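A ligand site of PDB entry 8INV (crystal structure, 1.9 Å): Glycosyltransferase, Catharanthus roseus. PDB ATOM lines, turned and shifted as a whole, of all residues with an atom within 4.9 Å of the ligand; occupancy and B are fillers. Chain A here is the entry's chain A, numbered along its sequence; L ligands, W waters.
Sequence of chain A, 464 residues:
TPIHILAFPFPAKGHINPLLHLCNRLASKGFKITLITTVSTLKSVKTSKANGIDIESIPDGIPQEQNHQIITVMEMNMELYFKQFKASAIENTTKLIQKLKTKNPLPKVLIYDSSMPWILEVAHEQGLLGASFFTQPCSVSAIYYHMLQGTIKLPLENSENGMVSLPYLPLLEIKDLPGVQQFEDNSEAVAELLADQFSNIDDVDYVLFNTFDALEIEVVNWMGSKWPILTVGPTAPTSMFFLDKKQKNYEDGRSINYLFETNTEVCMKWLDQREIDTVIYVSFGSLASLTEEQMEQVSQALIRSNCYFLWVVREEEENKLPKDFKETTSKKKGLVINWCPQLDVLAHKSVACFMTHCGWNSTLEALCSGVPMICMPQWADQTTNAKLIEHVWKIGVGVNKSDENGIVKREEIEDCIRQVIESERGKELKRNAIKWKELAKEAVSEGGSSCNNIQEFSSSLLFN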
ATOM      1  N   LYS A  13      24.284   6.640   1.216  1.00  0.00           N
ATOM      2  CA  LYS A  13      24.297   5.177   1.097  1.00  0.00           C
ATOM      3  C   LYS A  13      23.270   4.661   0.084  1.00  0.00           C
ATOM      4  O   LYS A  13      23.535   3.648  -0.586  1.00  0.00           O
ATOM      5  CB  LYS A  13      24.066   4.534   2.471  1.00  0.00           C
ATOM      6  CG  LYS A  13      25.293   4.705   3.394  1.00  0.00           C
ATOM      7  CD  LYS A  13      25.202   3.865   4.649  1.00  0.00           C
ATOM      8  CE  LYS A  13      26.428   4.086   5.527  1.00  0.00           C
ATOM      9  NZ  LYS A  13      26.801   5.533   5.601  1.00  0.00           N
ATOM     10  N   GLY A  14      22.109   5.297  -0.030  1.00  0.00           N
ATOM     11  CA  GLY A  14      21.104   4.857  -0.990  1.00  0.00           C
ATOM     12  C   GLY A  14      21.476   5.095  -2.446  1.00  0.00           C
ATOM     13  O   GLY A  14      20.756   4.647  -3.349  1.00  0.00           O
ATOM     14  N   ASN A  17      25.221   2.363  -2.626  1.00  0.00           N
ATOM     15  CA  ASN A  17      25.012   0.920  -2.620  1.00  0.00           C
ATOM     16  C   ASN A  17      24.489   0.365  -3.937  1.00  0.00           C
ATOM     17  O   ASN A  17      25.059  -0.638  -4.412  1.00  0.00           O
ATOM     18  CB  ASN A  17      24.080   0.542  -1.449  1.00  0.00           C
ATOM     19  CG  ASN A  17      24.769   0.661  -0.112  1.00  0.00           C
ATOM     20  OD1 ASN A  17      25.977   0.880  -0.036  1.00  0.00           O
ATOM     21  ND2 ASN A  17      23.993   0.483   0.963  1.00  0.00           N
ATOM     22  N   TYR A 258      28.995  -5.227   0.928  1.00  0.00           N
ATOM     23  CA  TYR A 258      28.886  -4.048   1.774  1.00  0.00           C
ATOM     24  C   TYR A 258      30.230  -3.353   1.921  1.00  0.00           C
ATOM     25  O   TYR A 258      31.285  -4.000   1.976  1.00  0.00           O
ATOM     26  CB  TYR A 258      28.326  -4.373   3.172  1.00  0.00           C
ATOM     27  CG  TYR A 258      27.109  -5.289   3.160  1.00  0.00           C
ATOM     28  CD1 TYR A 258      25.839  -4.782   2.915  1.00  0.00           C
ATOM     29  CD2 TYR A 258      27.239  -6.656   3.414  1.00  0.00           C
ATOM     30  CE1 TYR A 258      24.709  -5.614   2.912  1.00  0.00           C
ATOM     31  CE2 TYR A 258      26.130  -7.483   3.416  1.00  0.00           C
ATOM     32  CZ  TYR A 258      24.864  -6.969   3.165  1.00  0.00           C
ATOM     33  OH  TYR A 258      23.754  -7.810   3.167  1.00  0.00           O
ATOM     34  N   TYR A 281      11.372  -6.758  10.751  1.00  0.00           N
ATOM     35  CA  TYR A 281      12.566  -5.965  10.502  1.00  0.00           C
ATOM     36  C   TYR A 281      12.159  -4.508  10.360  1.00  0.00           C
ATOM     37  O   TYR A 281      11.178  -4.208   9.672  1.00  0.00           O
ATOM     38  CB  TYR A 281      13.279  -6.467   9.245  1.00  0.00           C
ATOM     39  CG  TYR A 281      14.420  -5.623   8.791  1.00  0.00           C
ATOM     40  CD1 TYR A 281      15.390  -5.163   9.678  1.00  0.00           C
ATOM     41  CD2 TYR A 281      14.551  -5.291   7.445  1.00  0.00           C
ATOM     42  CE1 TYR A 281      16.456  -4.376   9.238  1.00  0.00           C
ATOM     43  CE2 TYR A 281      15.604  -4.509   7.005  1.00  0.00           C
ATOM     44  CZ  TYR A 281      16.545  -4.054   7.899  1.00  0.00           C
ATOM     45  OH  TYR A 281      17.585  -3.263   7.425  1.00  0.00           O
ATOM     46  N   SER A 283      13.540  -0.536   9.692  1.00  0.00           N
ATOM     47  CA  SER A 283      14.632   0.375   9.397  1.00  0.00           C
ATOM     48  C   SER A 283      14.099   1.604   8.672  1.00  0.00           C
ATOM     49  O   SER A 283      13.234   1.496   7.793  1.00  0.00           O
ATOM     50  CB  SER A 283      15.705  -0.311   8.532  1.00  0.00           C
ATOM     51  OG  SER A 283      16.662   0.630   8.081  1.00  0.00           O
ATOM     52  N   GLY A 285      16.308   3.607   7.079  1.00  0.00           N
ATOM     53  CA  GLY A 285      17.298   3.919   6.085  1.00  0.00           C
ATOM     54  C   GLY A 285      18.508   4.636   6.666  1.00  0.00           C
ATOM     55  O   GLY A 285      18.792   4.627   7.868  1.00  0.00           O
ATOM     56  N   SER A 286      19.228   5.294   5.758  1.00  0.00           N
ATOM     57  CA  SER A 286      20.505   5.894   6.086  1.00  0.00           C
ATOM     58  C   SER A 286      20.408   7.370   6.428  1.00  0.00           C
ATOM     59  O   SER A 286      21.362   7.913   7.005  1.00  0.00           O
ATOM     60  CB  SER A 286      21.486   5.698   4.909  1.00  0.00           C
ATOM     61  OG  SER A 286      21.139   6.522   3.811  1.00  0.00           O
ATOM     62  N   LEU A 287      19.283   8.034   6.134  1.00  0.00           N
ATOM     63  CA  LEU A 287      19.180   9.478   6.314  1.00  0.00           C
ATOM     64  C   LEU A 287      18.026   9.929   7.190  1.00  0.00           C
ATOM     65  O   LEU A 287      18.198  10.846   8.002  1.00  0.00           O
ATOM     66  CB  LEU A 287      19.060  10.176   4.956  1.00  0.00           C
ATOM     67  CG  LEU A 287      20.184   9.935   3.957  1.00  0.00           C
ATOM     68  CD1 LEU A 287      19.766  10.415   2.579  1.00  0.00           C
ATOM     69  CD2 LEU A 287      21.461  10.611   4.391  1.00  0.00           C
ATOM     70  N   VAL A 312      16.995  -1.328  13.199  1.00  0.00           N
ATOM     71  CA  VAL A 312      18.179  -0.533  12.911  1.00  0.00           C
ATOM     72  C   VAL A 312      17.931   0.893  13.385  1.00  0.00           C
ATOM     73  O   VAL A 312      17.086   1.603  12.832  1.00  0.00           O
ATOM     74  CB  VAL A 312      18.532  -0.548  11.422  1.00  0.00           C
ATOM     75  CG1 VAL A 312      19.756   0.314  11.156  1.00  0.00           C
ATOM     76  CG2 VAL A 312      18.752  -1.964  10.937  1.00  0.00           C
ATOM     77  N   TRP A 339      23.388  -0.736  12.484  1.00  0.00           N
ATOM     78  CA  TRP A 339      23.389  -1.015  11.052  1.00  0.00           C
ATOM     79  C   TRP A 339      23.417  -2.530  10.903  1.00  0.00           C
ATOM     80  O   TRP A 339      23.973  -3.216  11.775  1.00  0.00           O
ATOM     81  CB  TRP A 339      24.602  -0.367  10.343  1.00  0.00           C
ATOM     82  CG  TRP A 339      24.415  -0.044   8.877  1.00  0.00           C
ATOM     83  CD1 TRP A 339      25.120  -0.562   7.833  1.00  0.00           C
ATOM     84  CD2 TRP A 339      23.472   0.869   8.308  1.00  0.00           C
ATOM     85  NE1 TRP A 339      24.670  -0.032   6.642  1.00  0.00           N
ATOM     86  CE2 TRP A 339      23.647   0.842   6.907  1.00  0.00           C
ATOM     87  CE3 TRP A 339      22.482   1.707   8.849  1.00  0.00           C
ATOM     88  CZ2 TRP A 339      22.900   1.639   6.033  1.00  0.00           C
ATOM     89  CZ3 TRP A 339      21.721   2.484   7.975  1.00  0.00           C
ATOM     90  CH2 TRP A 339      21.933   2.446   6.590  1.00  0.00           C
ATOM     91  N   CYS A 340      22.779  -3.049   9.862  1.00  0.00           N
ATOM     92  CA  CYS A 340      22.660  -4.484   9.657  1.00  0.00           C
ATOM     93  C   CYS A 340      23.024  -4.828   8.225  1.00  0.00           C
ATOM     94  O   CYS A 340      23.171  -3.928   7.374  1.00  0.00           O
ATOM     95  CB  CYS A 340      21.239  -4.972  10.030  1.00  0.00           C
ATOM     96  SG  CYS A 340      20.019  -4.790   8.731  1.00  0.00           S
ATOM     97  N   PRO A 341      23.252  -6.112   7.916  1.00  0.00           N
ATOM     98  CA  PRO A 341      23.438  -6.488   6.515  1.00  0.00           C
ATOM     99  C   PRO A 341      22.082  -6.663   5.845  1.00  0.00           C
ATOM    100  O   PRO A 341      21.504  -7.756   5.832  1.00  0.00           O
ATOM    101  CB  PRO A 341      24.253  -7.786   6.591  1.00  0.00           C
ATOM    102  CG  PRO A 341      23.782  -8.418   7.911  1.00  0.00           C
ATOM    103  CD  PRO A 341      23.453  -7.260   8.835  1.00  0.00           C
ATOM    104  N   GLN A 342      21.541  -5.557   5.315  1.00  0.00           N
ATOM    105  CA  GLN A 342      20.117  -5.538   5.004  1.00  0.00           C
ATOM    106  C   GLN A 342      19.741  -6.602   3.966  1.00  0.00           C
ATOM    107  O   GLN A 342      18.660  -7.177   4.041  1.00  0.00           O
ATOM    108  CB  GLN A 342      19.665  -4.143   4.533  1.00  0.00           C
ATOM    109  CG  GLN A 342      18.229  -4.154   3.921  1.00  0.00           C
ATOM    110  CD  GLN A 342      17.521  -2.796   3.893  1.00  0.00           C
ATOM    111  OE1 GLN A 342      17.024  -2.341   2.835  1.00  0.00           O
ATOM    112  NE2 GLN A 342      17.460  -2.131   5.040  1.00  0.00           N
ATOM    113  N   LEU A 343      20.609  -6.860   2.989  1.00  0.00           N
ATOM    114  CA  LEU A 343      20.264  -7.885   2.003  1.00  0.00           C
ATOM    115  C   LEU A 343      20.159  -9.255   2.653  1.00  0.00           C
ATOM    116  O   LEU A 343      19.251 -10.034   2.336  1.00  0.00           O
ATOM    117  CB  LEU A 343      21.297  -7.952   0.878  1.00  0.00           C
ATOM    118  CG  LEU A 343      21.557  -6.660   0.105  1.00  0.00           C
ATOM    119  CD1 LEU A 343      22.623  -6.916  -0.955  1.00  0.00           C
ATOM    120  CD2 LEU A 343      20.256  -6.216  -0.510  1.00  0.00           C
ATOM    121  N   HIS A 357      10.836   2.958   5.756  1.00  0.00           N
ATOM    122  CA  HIS A 357      10.549   4.315   5.300  1.00  0.00           C
ATOM    123  C   HIS A 357      10.258   4.385   3.805  1.00  0.00           C
ATOM    124  O   HIS A 357       9.900   5.451   3.319  1.00  0.00           O
ATOM    125  CB  HIS A 357      11.721   5.252   5.644  1.00  0.00           C
ATOM    126  CG  HIS A 357      12.909   5.116   4.749  1.00  0.00           C
ATOM    127  ND1 HIS A 357      13.508   3.909   4.472  1.00  0.00           N
ATOM    128  CD2 HIS A 357      13.640   6.061   4.094  1.00  0.00           C
ATOM    129  CE1 HIS A 357      14.549   4.107   3.676  1.00  0.00           C
ATOM    130  NE2 HIS A 357      14.646   5.401   3.429  1.00  0.00           N
ATOM    131  N   GLY A 359      12.297   4.025   1.155  1.00  0.00           N
ATOM    132  CA  GLY A 359      13.327   4.355   0.176  1.00  0.00           C
ATOM    133  C   GLY A 359      13.352   3.308  -0.924  1.00  0.00           C
ATOM    134  O   GLY A 359      12.943   2.167  -0.725  1.00  0.00           O
ATOM    135  N   TRP A 360      13.780   3.715  -2.125  1.00  0.00           N
ATOM    136  CA  TRP A 360      13.643   2.785  -3.251  1.00  0.00           C
ATOM    137  C   TRP A 360      14.487   1.518  -3.049  1.00  0.00           C
ATOM    138  O   TRP A 360      14.019   0.418  -3.361  1.00  0.00           O
ATOM    139  CB  TRP A 360      13.997   3.450  -4.589  1.00  0.00           C
ATOM    140  CG  TRP A 360      13.849   2.457  -5.728  1.00  0.00           C
ATOM    141  CD1 TRP A 360      14.811   2.103  -6.623  1.00  0.00           C
ATOM    142  CD2 TRP A 360      12.672   1.705  -6.068  1.00  0.00           C
ATOM    143  NE1 TRP A 360      14.317   1.155  -7.498  1.00  0.00           N
ATOM    144  CE2 TRP A 360      13.008   0.898  -7.183  1.00  0.00           C
ATOM    145  CE3 TRP A 360      11.381   1.628  -5.531  1.00  0.00           C
ATOM    146  CZ2 TRP A 360      12.092   0.045  -7.779  1.00  0.00           C
ATOM    147  CZ3 TRP A 360      10.470   0.768  -6.116  1.00  0.00           C
ATOM    148  CH2 TRP A 360      10.836  -0.021  -7.237  1.00  0.00           C
ATOM    149  N   ASN A 361      15.721   1.643  -2.531  1.00  0.00           N
ATOM    150  CA  ASN A 361      16.510   0.425  -2.365  1.00  0.00           C
ATOM    151  C   ASN A 361      15.835  -0.537  -1.412  1.00  0.00           C
ATOM    152  O   ASN A 361      15.761  -1.749  -1.668  1.00  0.00           O
ATOM    153  CB  ASN A 361      17.909   0.732  -1.851  1.00  0.00           C
ATOM    154  CG  ASN A 361      18.747   1.451  -2.855  1.00  0.00           C
ATOM    155  OD1 ASN A 361      19.171   0.868  -3.865  1.00  0.00           O
ATOM    156  ND2 ASN A 361      18.979   2.725  -2.611  1.00  0.00           N
ATOM    157  N   SER A 362      15.330  -0.026  -0.290  1.00  0.00           N
ATOM    158  CA  SER A 362      14.685  -0.898   0.669  1.00  0.00           C
ATOM    159  C   SER A 362      13.423  -1.517   0.074  1.00  0.00           C
ATOM    160  O   SER A 362      13.149  -2.715   0.295  1.00  0.00           O
ATOM    161  CB  SER A 362      14.367  -0.102   1.938  1.00  0.00           C
ATOM    162  OG  SER A 362      15.576   0.180   2.651  1.00  0.00           O
ATOM    163  N   GLU A 365      14.622  -4.124  -2.599  1.00  0.00           N
ATOM    164  CA  GLU A 365      15.239  -5.268  -1.934  1.00  0.00           C
ATOM    165  C   GLU A 365      14.199  -6.125  -1.213  1.00  0.00           C
ATOM    166  O   GLU A 365      14.284  -7.363  -1.238  1.00  0.00           O
ATOM    167  CB  GLU A 365      16.337  -4.793  -0.983  1.00  0.00           C
ATOM    168  CG  GLU A 365      17.575  -4.204  -1.740  1.00  0.00           C
ATOM    169  CD  GLU A 365      18.460  -3.316  -0.870  1.00  0.00           C
ATOM    170  OE1 GLU A 365      18.283  -3.315   0.362  1.00  0.00           O
ATOM    171  OE2 GLU A 365      19.356  -2.624  -1.415  1.00  0.00           O
ATOM    172  N   TRP A 379       9.791  11.317   3.439  1.00  0.00           N
ATOM    173  CA  TRP A 379       9.877  12.451   2.519  1.00  0.00           C
ATOM    174  C   TRP A 379      10.418  11.996   1.165  1.00  0.00           C
ATOM    175  O   TRP A 379      10.697  10.812   0.942  1.00  0.00           O
ATOM    176  CB  TRP A 379      10.761  13.577   3.098  1.00  0.00           C
ATOM    177  CG  TRP A 379      11.929  13.114   3.931  1.00  0.00           C
ATOM    178  CD1 TRP A 379      12.051  13.169   5.303  1.00  0.00           C
ATOM    179  CD2 TRP A 379      13.138  12.517   3.443  1.00  0.00           C
ATOM    180  NE1 TRP A 379      13.281  12.657   5.682  1.00  0.00           N
ATOM    181  CE2 TRP A 379      13.947  12.236   4.567  1.00  0.00           C
ATOM    182  CE3 TRP A 379      13.604  12.182   2.170  1.00  0.00           C
ATOM    183  CZ2 TRP A 379      15.219  11.662   4.446  1.00  0.00           C
ATOM    184  CZ3 TRP A 379      14.859  11.596   2.056  1.00  0.00           C
ATOM    185  CH2 TRP A 379      15.650  11.338   3.192  1.00  0.00           C
ATOM    186  N   GLN A 382       9.763   8.645  -1.063  1.00  0.00           N
ATOM    187  CA  GLN A 382       9.218   7.614  -0.175  1.00  0.00           C
ATOM    188  C   GLN A 382       7.689   7.611  -0.199  1.00  0.00           C
ATOM    189  O   GLN A 382       7.061   6.550  -0.128  1.00  0.00           O
ATOM    190  CB  GLN A 382       9.740   7.834   1.235  1.00  0.00           C
ATOM    191  CG  GLN A 382      11.247   7.682   1.320  1.00  0.00           C
ATOM    192  CD  GLN A 382      11.849   8.495   2.449  1.00  0.00           C
ATOM    193  OE1 GLN A 382      11.223   8.685   3.483  1.00  0.00           O
ATOM    194  NE2 GLN A 382      13.083   8.963   2.267  1.00  0.00           N
HETATM  195  N1  LIG L   1      20.914  -0.601   4.567  1.00  0.00           N
HETATM  196  C1  LIG L   1      21.768  -1.433   5.141  1.00  0.00           C
HETATM  197  N2  LIG L   1      21.724  -1.724   6.415  1.00  0.00           N
HETATM  198  C2  LIG L   1      20.808  -1.138   7.168  1.00  0.00           C
HETATM  199  C3  LIG L   1      19.881  -0.241   6.627  1.00  0.00           C
HETATM  200  C4  LIG L   1      19.967   0.017   5.264  1.00  0.00           C
HETATM  201  O1  LIG L   1      22.718  -2.065   4.346  1.00  0.00           O
HETATM  202  O2  LIG L   1      20.790  -1.445   8.510  1.00  0.00           O
HETATM  203  C5  LIG L   1      21.064  -0.298   3.133  1.00  0.00           C
HETATM  204  C6  LIG L   1      19.909  -0.746   2.236  1.00  0.00           C
HETATM  205  O3  LIG L   1      20.191  -2.019   1.827  1.00  0.00           O
HETATM  206  C7  LIG L   1      20.007   0.311   1.118  1.00  0.00           C
HETATM  207  C8  LIG L   1      20.358   1.448   1.690  1.00  0.00           C
HETATM  208  O4  LIG L   1      21.085   1.023   3.046  1.00  0.00           O
HETATM  209  O5  LIG L   1      21.110  -0.049   0.188  1.00  0.00           O
HETATM  210  C9  LIG L   1      19.160   2.324   2.061  1.00  0.00           C
HETATM  211  O6  LIG L   1      18.736   2.880   0.852  1.00  0.00           O
HETATM  212  P1  LIG L   1      17.204   3.406   0.664  1.00  0.00           P
HETATM  213  O7  LIG L   1      16.986   3.746  -0.789  1.00  0.00           O
HETATM  214  O8  LIG L   1      16.206   2.333   1.154  1.00  0.00           O
HETATM  215  O9  LIG L   1      16.924   4.664   1.657  1.00  0.00           O
HETATM  216  P2  LIG L   1      17.877   5.964   2.011  1.00  0.00           P
HETATM  217  O10 LIG L   1      18.512   6.422   0.704  1.00  0.00           O
HETATM  218  O11 LIG L   1      16.901   6.993   2.509  1.00  0.00           O
HETATM  219  O12 LIG L   1      18.920   5.589   3.054  1.00  0.00           O
HETATM  220  O   HOH W   1      21.953  -2.593  -0.874  1.00  0.00           O
HETATM  221  O   HOH W   2      16.570   9.169   0.654  1.00  0.00           O
HETATM  222  O   HOH W   3      20.905   7.689   0.715  1.00  0.00           O
HETATM  223  O   HOH W   4      22.728  -3.381   1.710  1.00  0.00           O
HETATM  224  O   HOH W   5      16.604   7.405   5.250  1.00  0.00           O
HETATM  225  O   HOH W   6      16.719   0.462   5.383  1.00  0.00           O
HETATM  226  O   HOH W   7      25.221  -0.573   3.708  1.00  0.00           O
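A ring nitrogen (NE2) of His 357 lies within hydrogen-bond range of an oxygen (O11) of the ligand (2.9 Å).
The backbone NH (N) of Ser 286 is in hydrogen-bond range of an oxygen (O12) of the ligand (2.7 Å).
OE1 of Glu 365 lies within hydrogen-bond range of O3 of the ligand.
The backbone NH of Cys 340 lies within hydrogen-bond range of an oxygen (O2) of the ligand, at 2.9 Å.
The side-chain amide oxygen of Gln 342 lies within hydrogen-bond range of an oxygen (O3) of the ligand.
The side-chain sulfur (SG) of Cys 340 lies within hydrogen-bond range of an oxygen (O2) of the ligand (3.4 Å).
The side-chain amide nitrogen (ND2) of Asn 361 lies within hydrogen-bond range of an oxygen (O7) of the ligand.
N of Asn 361 sits at hydrogen-bond distance from O7 of the ligand, 3.0 Å away.
An oxygen (O7) of the ligand sits at hydrogen-bond distance from the backbone NH (N) of Trp 360, 3.5 Å away.
The side-chain hydroxyl (OG) of Ser 362 sits at hydrogen-bond distance from an oxygen (O8) of the ligand.
The side-chain hydroxyl (OG) of Ser 286 sits at hydrogen-bond distance from an oxygen (O12) of the ligand (2.5 Å).
The backbone NH (N) of Ser 362 sits at hydrogen-bond distance from an oxygen (O8) of the ligand.
A nitrogen (N2) of the ligand is in hydrogen-bond range of the backbone carbonyl oxygen (O) of Cys 340 (2.8 Å).
ND2 of Asn 17 is in hydrogen-bond range of O5 of the ligand (3.0 Å).
Water W3 lies within hydrogen-bond range of O10 of the ligand (2.7 Å), N of Gly 14 (2.8 Å) and OG of Ser 286 (3.3 Å).
Water W5 lies within hydrogen-bond range of an oxygen (O11) of the ligand, the backbone NH of Leu 287, a ring nitrogen (NE2) of His 357 and the backbone NH of Ser 286.
Water W1 lies within hydrogen-bond range of the side-chain carboxylate (OE2) of Glu 365 and an oxygen (O5) of the ligand.
Water W7 lies within hydrogen-bond range of O1 of the ligand (3.0 Å), NE1 of Trp 339 (3.0 Å) and ND2 of Asn 17 (3.2 Å).
Water W6 lies within hydrogen-bond range of the side-chain hydroxyl (OG) of Ser 283 (2.7 Å), the side-chain amide nitrogen (NE2) of Gln 342 (2.7 Å) and the side-chain hydroxyl (OG) of Ser 362 (3.0 Å).
The backbone carbonyl oxygen of Gly 14 sits at hydrogen-bond distance from the side-chain amide nitrogen of Asn 361 (2.7 Å).
The side-chain amide oxygen (OE1) of Gln 382 lies close to the backbone carbonyl oxygen (O) of His 357, 3.5 Å away.
The side-chain sulfur (SG) of Cys 340 lies within hydrogen-bond range of the side-chain hydroxyl (OH) of Tyr 281.
The side-chain carboxylate of Glu 365 lies close to the side-chain amide oxygen of Gln 342 (2.9 Å).
N of His 357 is in hydrogen-bond range of O of Ser 283, at 3.5 Å.
The side-chain amide nitrogen (NE2) of Gln 342 sits at hydrogen-bond distance from the side-chain hydroxyl (OH) of Tyr 281 (2.6 Å).
OG of Ser 283 sits at hydrogen-bond distance from N of Gly 285 (3.2 Å).
OG of Ser 362 is in hydrogen-bond range of OE1 of Gln 342 (2.9 Å).
NE1 of Trp 339 sits close to N2 of the ligand, 3.4 Å away.
Merely in contact with the ligand: Gly 14 (3.5 Å), Tyr 281 (3.8 Å), Ser 283 (3.6 Å), Gly 285 (3.8 Å), Leu 287 (3.9 Å), Val 312 (3.2 Å) and Gly 359 (3.7 Å).
Of the 23 residues printed, 17 come within 4 Å of the ligand.
The nearest printed residue that does not touch the ligand is Gln 382 (4.3 Å).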
